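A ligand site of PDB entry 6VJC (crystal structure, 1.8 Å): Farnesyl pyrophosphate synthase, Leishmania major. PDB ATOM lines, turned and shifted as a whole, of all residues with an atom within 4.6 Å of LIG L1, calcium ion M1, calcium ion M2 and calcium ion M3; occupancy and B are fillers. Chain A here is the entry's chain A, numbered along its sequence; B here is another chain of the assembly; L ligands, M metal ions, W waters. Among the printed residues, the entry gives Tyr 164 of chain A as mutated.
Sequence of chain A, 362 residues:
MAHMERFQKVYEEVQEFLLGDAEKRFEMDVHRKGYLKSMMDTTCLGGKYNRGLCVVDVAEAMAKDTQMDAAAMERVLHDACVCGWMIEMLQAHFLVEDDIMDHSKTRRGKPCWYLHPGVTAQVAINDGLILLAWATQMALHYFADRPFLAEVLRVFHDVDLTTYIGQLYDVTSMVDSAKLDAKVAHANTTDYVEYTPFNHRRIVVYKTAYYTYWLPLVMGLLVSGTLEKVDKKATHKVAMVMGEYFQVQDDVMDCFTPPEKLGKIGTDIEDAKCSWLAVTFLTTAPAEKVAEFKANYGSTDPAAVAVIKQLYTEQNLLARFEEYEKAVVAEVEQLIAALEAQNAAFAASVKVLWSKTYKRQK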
ATOM      1  N   PHE A  94     -17.905   8.613  27.373  1.00  0.00           N
ATOM      2  CA  PHE A  94     -17.257   9.793  26.776  1.00  0.00           C
ATOM      3  C   PHE A  94     -15.968  10.085  27.559  1.00  0.00           C
ATOM      4  O   PHE A  94     -14.955  10.334  26.921  1.00  0.00           O
ATOM      5  CB  PHE A  94     -18.172  11.017  26.802  1.00  0.00           C
ATOM      6  CG  PHE A  94     -19.327  11.065  25.832  1.00  0.00           C
ATOM      7  CD1 PHE A  94     -19.297  10.433  24.591  1.00  0.00           C
ATOM      8  CD2 PHE A  94     -20.431  11.824  26.148  1.00  0.00           C
ATOM      9  CE1 PHE A  94     -20.368  10.541  23.723  1.00  0.00           C
ATOM     10  CE2 PHE A  94     -21.531  11.897  25.292  1.00  0.00           C
ATOM     11  CZ  PHE A  94     -21.483  11.286  24.056  1.00  0.00           C
ATOM     12  N   LEU A  95     -16.004   9.989  28.878  1.00  0.00           N
ATOM     13  CA  LEU A  95     -14.826  10.378  29.697  1.00  0.00           C
ATOM     14  C   LEU A  95     -13.765   9.285  29.569  1.00  0.00           C
ATOM     15  O   LEU A  95     -12.580   9.625  29.530  1.00  0.00           O
ATOM     16  CB  LEU A  95     -15.250  10.637  31.131  1.00  0.00           C
ATOM     17  CG  LEU A  95     -16.310  11.738  31.322  1.00  0.00           C
ATOM     18  CD1 LEU A  95     -16.392  12.088  32.802  1.00  0.00           C
ATOM     19  CD2 LEU A  95     -15.955  12.989  30.533  1.00  0.00           C
ATOM     20  N   GLU A  97     -13.063   7.412  26.921  1.00  0.00           N
ATOM     21  CA  GLU A  97     -12.464   7.577  25.586  1.00  0.00           C
ATOM     22  C   GLU A  97     -11.693   8.910  25.554  1.00  0.00           C
ATOM     23  O   GLU A  97     -10.559   8.948  25.012  1.00  0.00           O
ATOM     24  CB  GLU A  97     -13.539   7.529  24.504  1.00  0.00           C
ATOM     25  CG  GLU A  97     -14.327   6.217  24.415  1.00  0.00           C
ATOM     26  CD  GLU A  97     -13.564   4.910  24.265  1.00  0.00           C
ATOM     27  OE1 GLU A  97     -12.334   4.933  24.018  1.00  0.00           O
ATOM     28  OE2 GLU A  97     -14.223   3.824  24.335  1.00  0.00           O
ATOM     29  N   ASP A  98     -12.250   9.968  26.110  1.00  0.00           N
ATOM     30  CA  ASP A  98     -11.590  11.300  26.087  1.00  0.00           C
ATOM     31  C   ASP A  98     -10.308  11.256  26.928  1.00  0.00           C
ATOM     32  O   ASP A  98      -9.297  11.859  26.530  1.00  0.00           O
ATOM     33  CB  ASP A  98     -12.520  12.418  26.531  1.00  0.00           C
ATOM     34  CG  ASP A  98     -11.809  13.769  26.486  1.00  0.00           C
ATOM     35  OD1 ASP A  98     -11.447  14.178  25.395  1.00  0.00           O
ATOM     36  OD2 ASP A  98     -11.509  14.283  27.568  1.00  0.00           O
ATOM     37  N   ASP A  99     -10.314  10.554  28.055  1.00  0.00           N
ATOM     38  CA  ASP A  99      -9.130  10.501  28.955  1.00  0.00           C
ATOM     39  C   ASP A  99      -8.002   9.806  28.173  1.00  0.00           C
ATOM     40  O   ASP A  99      -6.824  10.157  28.350  1.00  0.00           O
ATOM     41  CB  ASP A  99      -9.497   9.844  30.295  1.00  0.00           C
ATOM     42  CG  ASP A  99     -10.188  10.797  31.257  1.00  0.00           C
ATOM     43  OD1 ASP A  99     -10.098  12.054  31.053  1.00  0.00           O
ATOM     44  OD2 ASP A  99     -10.793  10.309  32.224  1.00  0.00           O
ATOM     45  N   MET A 101      -7.795   9.856  24.745  1.00  0.00           N
ATOM     46  CA  MET A 101      -7.431  10.767  23.637  1.00  0.00           C
ATOM     47  C   MET A 101      -6.557  11.926  24.167  1.00  0.00           C
ATOM     48  O   MET A 101      -5.624  12.337  23.438  1.00  0.00           O
ATOM     49  CB  MET A 101      -8.688  11.287  22.939  1.00  0.00           C
ATOM     50  CG  MET A 101      -9.378  10.174  22.120  1.00  0.00           C
ATOM     51  SD  MET A 101     -10.847  10.867  21.328  1.00  0.00           S
ATOM     52  CE  MET A 101     -12.161  10.028  22.170  1.00  0.00           C
ATOM     53  N   ASP A 102      -6.836  12.421  25.376  1.00  0.00           N
ATOM     54  CA  ASP A 102      -6.122  13.565  25.978  1.00  0.00           C
ATOM     55  C   ASP A 102      -4.887  13.078  26.761  1.00  0.00           C
ATOM     56  O   ASP A 102      -4.075  13.953  27.201  1.00  0.00           O
ATOM     57  CB  ASP A 102      -7.021  14.375  26.900  1.00  0.00           C
ATOM     58  CG  ASP A 102      -8.023  15.271  26.158  1.00  0.00           C
ATOM     59  OD1 ASP A 102      -7.919  15.422  24.908  1.00  0.00           O
ATOM     60  OD2 ASP A 102      -8.922  15.739  26.831  1.00  0.00           O
ATOM     61  N   SER A 104      -4.752  11.780  29.747  1.00  0.00           N
ATOM     62  CA  SER A 104      -4.933  12.494  31.028  1.00  0.00           C
ATOM     63  C   SER A 104      -4.567  11.560  32.203  1.00  0.00           C
ATOM     64  O   SER A 104      -4.417  10.313  32.006  1.00  0.00           O
ATOM     65  CB  SER A 104      -6.346  13.036  31.166  1.00  0.00           C
ATOM     66  OG  SER A 104      -6.616  14.017  30.174  1.00  0.00           O
ATOM     67  N   ARG A 107      -9.290  11.511  36.968  1.00  0.00           N
ATOM     68  CA  ARG A 107     -10.715  11.780  36.686  1.00  0.00           C
ATOM     69  C   ARG A 107     -11.495  11.536  37.975  1.00  0.00           C
ATOM     70  O   ARG A 107     -11.342  10.453  38.577  1.00  0.00           O
ATOM     71  CB  ARG A 107     -11.227  10.882  35.548  1.00  0.00           C
ATOM     72  CG  ARG A 107     -12.748  10.859  35.374  1.00  0.00           C
ATOM     73  CD  ARG A 107     -13.222  12.197  34.794  1.00  0.00           C
ATOM     74  NE  ARG A 107     -12.763  12.388  33.428  1.00  0.00           N
ATOM     75  CZ  ARG A 107     -12.906  13.509  32.732  1.00  0.00           C
ATOM     76  NH1 ARG A 107     -13.604  14.524  33.234  1.00  0.00           N
ATOM     77  NH2 ARG A 107     -12.454  13.576  31.485  1.00  0.00           N
ATOM     78  N   THR A 163     -22.050  14.656  19.713  1.00  0.00           N
ATOM     79  CA  THR A 163     -20.902  14.798  20.646  1.00  0.00           C
ATOM     80  C   THR A 163     -19.606  14.405  19.908  1.00  0.00           C
ATOM     81  O   THR A 163     -18.569  15.075  20.171  1.00  0.00           O
ATOM     82  CB  THR A 163     -21.108  13.964  21.909  1.00  0.00           C
ATOM     83  OG1 THR A 163     -22.396  14.300  22.453  1.00  0.00           O
ATOM     84  CG2 THR A 163     -19.994  14.203  22.908  1.00  0.00           C
ATOM     85  N   TYR A 164     -19.594  13.348  19.097  1.00  0.00           N
ATOM     86  CA  TYR A 164     -18.366  12.908  18.363  1.00  0.00           C
ATOM     87  C   TYR A 164     -17.990  13.982  17.317  1.00  0.00           C
ATOM     88  O   TYR A 164     -16.816  14.147  17.050  1.00  0.00           O
ATOM     89  CB  TYR A 164     -18.535  11.535  17.697  1.00  0.00           C
ATOM     90  CG  TYR A 164     -18.904  10.400  18.630  1.00  0.00           C
ATOM     91  CD1 TYR A 164     -18.323  10.266  19.877  1.00  0.00           C
ATOM     92  CD2 TYR A 164     -19.875   9.486  18.277  1.00  0.00           C
ATOM     93  CE1 TYR A 164     -18.724   9.271  20.751  1.00  0.00           C
ATOM     94  CE2 TYR A 164     -20.251   8.469  19.119  1.00  0.00           C
ATOM     95  CZ  TYR A 164     -19.704   8.370  20.380  1.00  0.00           C
ATOM     96  OH  TYR A 164     -20.105   7.374  21.263  1.00  0.00           O
ATOM     97  N   GLN A 167     -16.342  16.581  19.219  1.00  0.00           N
ATOM     98  CA  GLN A 167     -14.995  16.034  19.533  1.00  0.00           C
ATOM     99  C   GLN A 167     -14.063  16.137  18.305  1.00  0.00           C
ATOM    100  O   GLN A 167     -12.879  16.514  18.509  1.00  0.00           O
ATOM    101  CB  GLN A 167     -15.082  14.601  20.042  1.00  0.00           C
ATOM    102  CG  GLN A 167     -13.731  14.063  20.481  1.00  0.00           C
ATOM    103  CD  GLN A 167     -13.253  14.573  21.838  1.00  0.00           C
ATOM    104  OE1 GLN A 167     -13.718  15.599  22.327  1.00  0.00           O
ATOM    105  NE2 GLN A 167     -12.350  13.838  22.487  1.00  0.00           N
ATOM    106  N   ASP A 170     -12.965  19.654  18.240  1.00  0.00           N
ATOM    107  CA  ASP A 170     -12.035  19.812  19.377  1.00  0.00           C
ATOM    108  C   ASP A 170     -10.641  19.263  18.989  1.00  0.00           C
ATOM    109  O   ASP A 170      -9.638  20.018  19.162  1.00  0.00           O
ATOM    110  CB  ASP A 170     -12.563  19.125  20.642  1.00  0.00           C
ATOM    111  CG  ASP A 170     -11.616  19.267  21.819  1.00  0.00           C
ATOM    112  OD1 ASP A 170     -10.510  18.693  21.722  1.00  0.00           O
ATOM    113  OD2 ASP A 170     -11.937  20.002  22.750  1.00  0.00           O
ATOM    114  N   LYS A 207     -19.855  19.460  21.333  1.00  0.00           N
ATOM    115  CA  LYS A 207     -19.206  18.460  22.210  1.00  0.00           C
ATOM    116  C   LYS A 207     -19.889  18.421  23.590  1.00  0.00           C
ATOM    117  O   LYS A 207     -19.815  17.373  24.241  1.00  0.00           O
ATOM    118  CB  LYS A 207     -17.698  18.644  22.332  1.00  0.00           C
ATOM    119  CG  LYS A 207     -17.201  19.605  23.397  1.00  0.00           C
ATOM    120  CD  LYS A 207     -15.692  19.534  23.635  1.00  0.00           C
ATOM    121  CE  LYS A 207     -15.274  20.613  24.631  1.00  0.00           C
ATOM    122  NZ  LYS A 207     -13.814  20.580  24.922  1.00  0.00           N
ATOM    123  N   THR A 208     -20.534  19.501  24.039  1.00  0.00           N
ATOM    124  CA  THR A 208     -21.024  19.577  25.441  1.00  0.00           C
ATOM    125  C   THR A 208     -22.519  19.883  25.547  1.00  0.00           C
ATOM    126  O   THR A 208     -23.172  19.208  26.340  1.00  0.00           O
ATOM    127  CB  THR A 208     -20.239  20.616  26.257  1.00  0.00           C
ATOM    128  OG1 THR A 208     -18.891  20.131  26.286  1.00  0.00           O
ATOM    129  CG2 THR A 208     -20.827  20.806  27.660  1.00  0.00           C
ATOM    130  N   TYR A 211     -25.470  16.911  24.903  1.00  0.00           N
ATOM    131  CA  TYR A 211     -25.606  15.766  25.829  1.00  0.00           C
ATOM    132  C   TYR A 211     -25.733  16.229  27.284  1.00  0.00           C
ATOM    133  O   TYR A 211     -26.307  15.462  28.059  1.00  0.00           O
ATOM    134  CB  TYR A 211     -24.446  14.781  25.661  1.00  0.00           C
ATOM    135  CG  TYR A 211     -23.231  14.960  26.527  1.00  0.00           C
ATOM    136  CD1 TYR A 211     -22.188  15.763  26.109  1.00  0.00           C
ATOM    137  CD2 TYR A 211     -23.032  14.181  27.672  1.00  0.00           C
ATOM    138  CE1 TYR A 211     -21.001  15.843  26.840  1.00  0.00           C
ATOM    139  CE2 TYR A 211     -21.856  14.248  28.410  1.00  0.00           C
ATOM    140  CZ  TYR A 211     -20.836  15.089  27.996  1.00  0.00           C
ATOM    141  OH  TYR A 211     -19.654  15.153  28.694  1.00  0.00           O
ATOM    142  N   GLN A 247     -19.479  24.790  29.430  1.00  0.00           N
ATOM    143  CA  GLN A 247     -18.138  24.405  28.894  1.00  0.00           C
ATOM    144  C   GLN A 247     -17.144  25.575  29.020  1.00  0.00           C
ATOM    145  O   GLN A 247     -15.966  25.349  29.232  1.00  0.00           O
ATOM    146  CB  GLN A 247     -18.214  23.956  27.439  1.00  0.00           C
ATOM    147  CG  GLN A 247     -16.906  23.401  26.928  1.00  0.00           C
ATOM    148  CD  GLN A 247     -16.445  22.239  27.765  1.00  0.00           C
ATOM    149  OE1 GLN A 247     -17.209  21.336  28.021  1.00  0.00           O
ATOM    150  NE2 GLN A 247     -15.184  22.260  28.176  1.00  0.00           N
ATOM    151  N   ASP A 250     -15.868  25.201  32.440  1.00  0.00           N
ATOM    152  CA  ASP A 250     -14.928  24.059  32.422  1.00  0.00           C
ATOM    153  C   ASP A 250     -13.568  24.544  31.878  1.00  0.00           C
ATOM    154  O   ASP A 250     -12.536  24.192  32.439  1.00  0.00           O
ATOM    155  CB  ASP A 250     -15.528  22.920  31.619  1.00  0.00           C
ATOM    156  CG  ASP A 250     -14.668  21.689  31.719  1.00  0.00           C
ATOM    157  OD1 ASP A 250     -14.685  21.084  32.811  1.00  0.00           O
ATOM    158  OD2 ASP A 250     -13.954  21.404  30.732  1.00  0.00           O
ATOM    159  N   LYS A 264      -9.575  16.542  38.456  1.00  0.00           N
ATOM    160  CA  LYS A 264      -8.912  16.194  37.175  1.00  0.00           C
ATOM    161  C   LYS A 264      -7.821  17.207  36.914  1.00  0.00           C
ATOM    162  O   LYS A 264      -7.933  18.315  37.448  1.00  0.00           O
ATOM    163  CB  LYS A 264      -9.899  16.198  36.011  1.00  0.00           C
ATOM    164  CG  LYS A 264     -10.643  17.496  35.762  1.00  0.00           C
ATOM    165  CD  LYS A 264     -11.800  17.379  34.802  1.00  0.00           C
ATOM    166  CE  LYS A 264     -12.381  18.750  34.504  1.00  0.00           C
ATOM    167  NZ  LYS A 264     -13.644  18.660  33.741  1.00  0.00           N
ATOM    168  N   ASP A 268      -5.160  21.814  28.794  1.00  0.00           N
ATOM    169  CA  ASP A 268      -5.581  22.617  27.639  1.00  0.00           C
ATOM    170  C   ASP A 268      -4.372  23.443  27.171  1.00  0.00           C
ATOM    171  O   ASP A 268      -4.214  23.632  25.956  1.00  0.00           O
ATOM    172  CB  ASP A 268      -6.737  23.545  27.960  1.00  0.00           C
ATOM    173  CG  ASP A 268      -8.078  22.865  28.122  1.00  0.00           C
ATOM    174  OD1 ASP A 268      -8.143  21.632  27.863  1.00  0.00           O
ATOM    175  OD2 ASP A 268      -9.063  23.599  28.467  1.00  0.00           O
ATOM    176  N   ASN B 126     -12.013   8.490  17.956  1.00  0.00           N
ATOM    177  CA  ASN B 126     -13.235   9.285  17.734  1.00  0.00           C
ATOM    178  C   ASN B 126     -13.742   9.061  16.304  1.00  0.00           C
ATOM    179  O   ASN B 126     -14.957   9.016  16.108  1.00  0.00           O
ATOM    180  CB  ASN B 126     -12.976  10.764  18.020  1.00  0.00           C
ATOM    181  CG  ASN B 126     -14.270  11.558  18.055  1.00  0.00           C
ATOM    182  OD1 ASN B 126     -15.100  11.324  18.922  1.00  0.00           O
ATOM    183  ND2 ASN B 126     -14.437  12.451  17.089  1.00  0.00           N
HETATM  184  O1  LIG L   1     -13.739  16.775  31.585  1.00  0.00           O
HETATM  185  P1  LIG L   1     -12.693  17.203  30.585  1.00  0.00           P
HETATM  186  O2  LIG L   1     -11.696  16.087  30.333  1.00  0.00           O
HETATM  187  O3  LIG L   1     -11.998  18.434  30.976  1.00  0.00           O
HETATM  188  C1  LIG L   1     -13.603  17.581  29.019  1.00  0.00           C
HETATM  189  P2  LIG L   1     -12.579  18.327  27.717  1.00  0.00           P
HETATM  190  O4  LIG L   1     -11.434  17.420  27.388  1.00  0.00           O
HETATM  191  O5  LIG L   1     -13.466  18.506  26.475  1.00  0.00           O
HETATM  192  O6  LIG L   1     -12.104  19.643  28.212  1.00  0.00           O
HETATM  193  C2  LIG L   1     -14.220  16.247  28.617  1.00  0.00           C
HETATM  194  N1  LIG L   1     -15.253  16.288  27.567  1.00  0.00           N
HETATM  195  C3  LIG L   1     -15.334  15.225  26.693  1.00  0.00           C
HETATM  196  C4  LIG L   1     -16.355  15.122  25.771  1.00  0.00           C
HETATM  197  C5  LIG L   1     -17.178  16.227  25.600  1.00  0.00           C
HETATM  198  C6  LIG L   1     -17.085  17.294  26.456  1.00  0.00           C
HETATM  199  C7  LIG L   1     -16.109  17.307  27.458  1.00  0.00           C
HETATM  200  C8  LIG L   1     -16.611  13.824  25.048  1.00  0.00           C
HETATM  201  C9  LIG L   1     -15.929  13.586  23.728  1.00  0.00           C
HETATM  202  C10 LIG L   1     -16.253  12.239  23.080  1.00  0.00           C
HETATM  203  C11 LIG L   1     -15.201  11.195  23.247  1.00  0.00           C
HETATM  204  P1  LG2 L   2     -18.955  14.741  36.167  1.00  0.00           P
HETATM  205  O1  LG2 L   2     -17.701  14.180  36.744  1.00  0.00           O
HETATM  206  O2  LG2 L   2     -19.879  15.609  37.097  1.00  0.00           O
HETATM  207  O3  LG2 L   2     -19.828  13.749  35.381  1.00  0.00           O
HETATM  208  O4  LG2 L   2     -18.354  15.704  34.992  1.00  0.00           O
HETATM  209  P2  LG2 L   2     -18.898  17.075  34.309  1.00  0.00           P
HETATM  210  O5  LG2 L   2     -18.187  18.301  34.906  1.00  0.00           O
HETATM  211  O6  LG2 L   2     -20.374  17.168  34.366  1.00  0.00           O
HETATM  212  O7  LG2 L   2     -18.514  16.840  32.783  1.00  0.00           O
HETATM  213  C1  LG2 L   2     -17.170  16.668  32.368  1.00  0.00           C
HETATM  214  C2  LG2 L   2     -17.126  16.839  30.860  1.00  0.00           C
HETATM  215  C3  LG2 L   2     -17.509  18.237  30.333  1.00  0.00           C
HETATM  216  C4  LG2 L   2     -18.720  18.311  29.474  1.00  0.00           C
HETATM  217  C5  LG2 L   2     -16.894  19.458  30.969  1.00  0.00           C
HETATM  218 CA    CA M   1     -11.791  20.670  30.252  1.00  0.00          CA
HETATM  219 CA    CA M   2     -10.185  15.834  28.683  1.00  0.00          CA
HETATM  220 CA    CA M   3     -10.664  16.449  25.306  1.00  0.00          CA
HETATM  221  O   HOH W   1     -10.138  18.777  24.728  1.00  0.00           O
HETATM  222  O   HOH W   2      -9.122  14.101  29.746  1.00  0.00           O
HETATM  223  O   HOH W   3      -9.406  20.738  30.112  1.00  0.00           O
HETATM  224  O   HOH W   4     -11.478  22.685  29.100  1.00  0.00           O
HETATM  225  O   HOH W   5     -10.298  16.154  22.968  1.00  0.00           O
HETATM  226  O   HOH W   6     -11.469  21.604  32.583  1.00  0.00           O
HETATM  227  O   HOH W   7      -9.605  18.367  32.398  1.00  0.00           O
HETATM  228  O   HOH W   8     -12.874  16.827  24.454  1.00  0.00           O
HETATM  229  O   HOH W   9      -8.753  17.324  29.676  1.00  0.00           O
HETATM  230  O   HOH W  10     -10.408  20.870  26.463  1.00  0.00           O
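The nearest printed residue that does not touch calcium ion M2 is Arg 107 (4.3 Å).
Calcium ion M3 is bound by water W5, water W8, OD1 of Asp 98, OD2 of Asp 102, O4 of LIG L1 and water W1.
Calcium ion M3 has six donor atoms within binding distance.
Slightly farther from calcium ion M3 lies the side-chain carboxylate (OD1) of Asp 102 (3.0 Å).
The side-chain amino group (NZ) of Lys 207 lies within salt-bridge range of an oxygen (O5) of LIG L1 (2.6 Å).
The guanidinium group (NH1) of Arg 107 is in salt-bridge range of an oxygen (O1) of LIG L1 (2.8 Å).
NZ of Lys 264 lies within salt-bridge range of O1 of LIG L1 (2.9 Å).
The side-chain amide nitrogen (NE2) of Gln 167 sits close to the side-chain carboxylate (OD1) of Asp 98, 3.1 Å away.
The side-chain amino group of Lys 264 is in salt-bridge range of the side-chain carboxylate of Asp 250.
The side-chain amide nitrogen (NE2) of Gln 247 sits close to the side-chain carboxylate (OD2) of Asp 250, 3.0 Å away.
NZ of Lys 207 is in salt-bridge range of OD2 of Asp 170 (2.9 Å).
NH2 of Arg 107 is in salt-bridge range of OD1 of Asp 99 (2.8 Å).
The side-chain sulfur (SD) of Met 101 is in hydrogen-bond range of the side-chain amide nitrogen (NE2) of Gln 167 (3.5 Å).
The side-chain hydroxyl (OG1) of Thr 208 sits at hydrogen-bond distance from the side-chain amide oxygen (OE1) of Gln 247 (2.7 Å).
Of the 21 residues printed, 1 comes within 4 Å of calcium ion M1.
Water W2 lies within hydrogen-bond range of OG of Ser 104 (2.5 Å) and OD1 of Asp 99 (2.6 Å).
Water W8 lies within hydrogen-bond range of OE1 of Gln 167 (2.6 Å) and O5 of LIG L1 (2.7 Å).
Water W5 lies within hydrogen-bond range of the side-chain carboxylate (OD1) of Asp 170, the side-chain amide nitrogen (NE2) of Gln 167 and the side-chain carboxylate (OD1) of Asp 102.
Calcium ion M1 is bound by an oxygen (O6) of LIG L1 (2.3 Å), the side-chain carboxylate of Asp 250 (2.3 Å), water W4 (2.3 Å), an oxygen (O3) of LIG L1 (2.4 Å), water W3 (2.4 Å) and water W6 (2.5 Å).
CB of Phe 94 touches C8 of LIG L1, 3.7 Å away.
Met 101 touches LIG L1 (CE to C11, 3.4 Å).
OE1 of Gln 167 touches C9 of LIG L1, at 3.3 Å.
OG1 of Thr 208 touches C6 of LIG L1, 3.4 Å away.
Ten residues have an atom within 4 Å of LIG L1: Phe 94, Asp 98, Met 101, Asp 102, Arg 107, Gln 167, Lys 207, Thr 208, Asp 250 and Lys 264.
Calcium ion M2 is bound by OD2 of Asp 102 (2.2 Å), O2 of LIG L1 (2.3 Å), water W9 (2.3 Å), water W2 (2.3 Å), OD2 of Asp 98 (2.3 Å) and O4 of LIG L1 (2.4 Å).
Calcium ion M2 has six donor atoms within binding distance.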
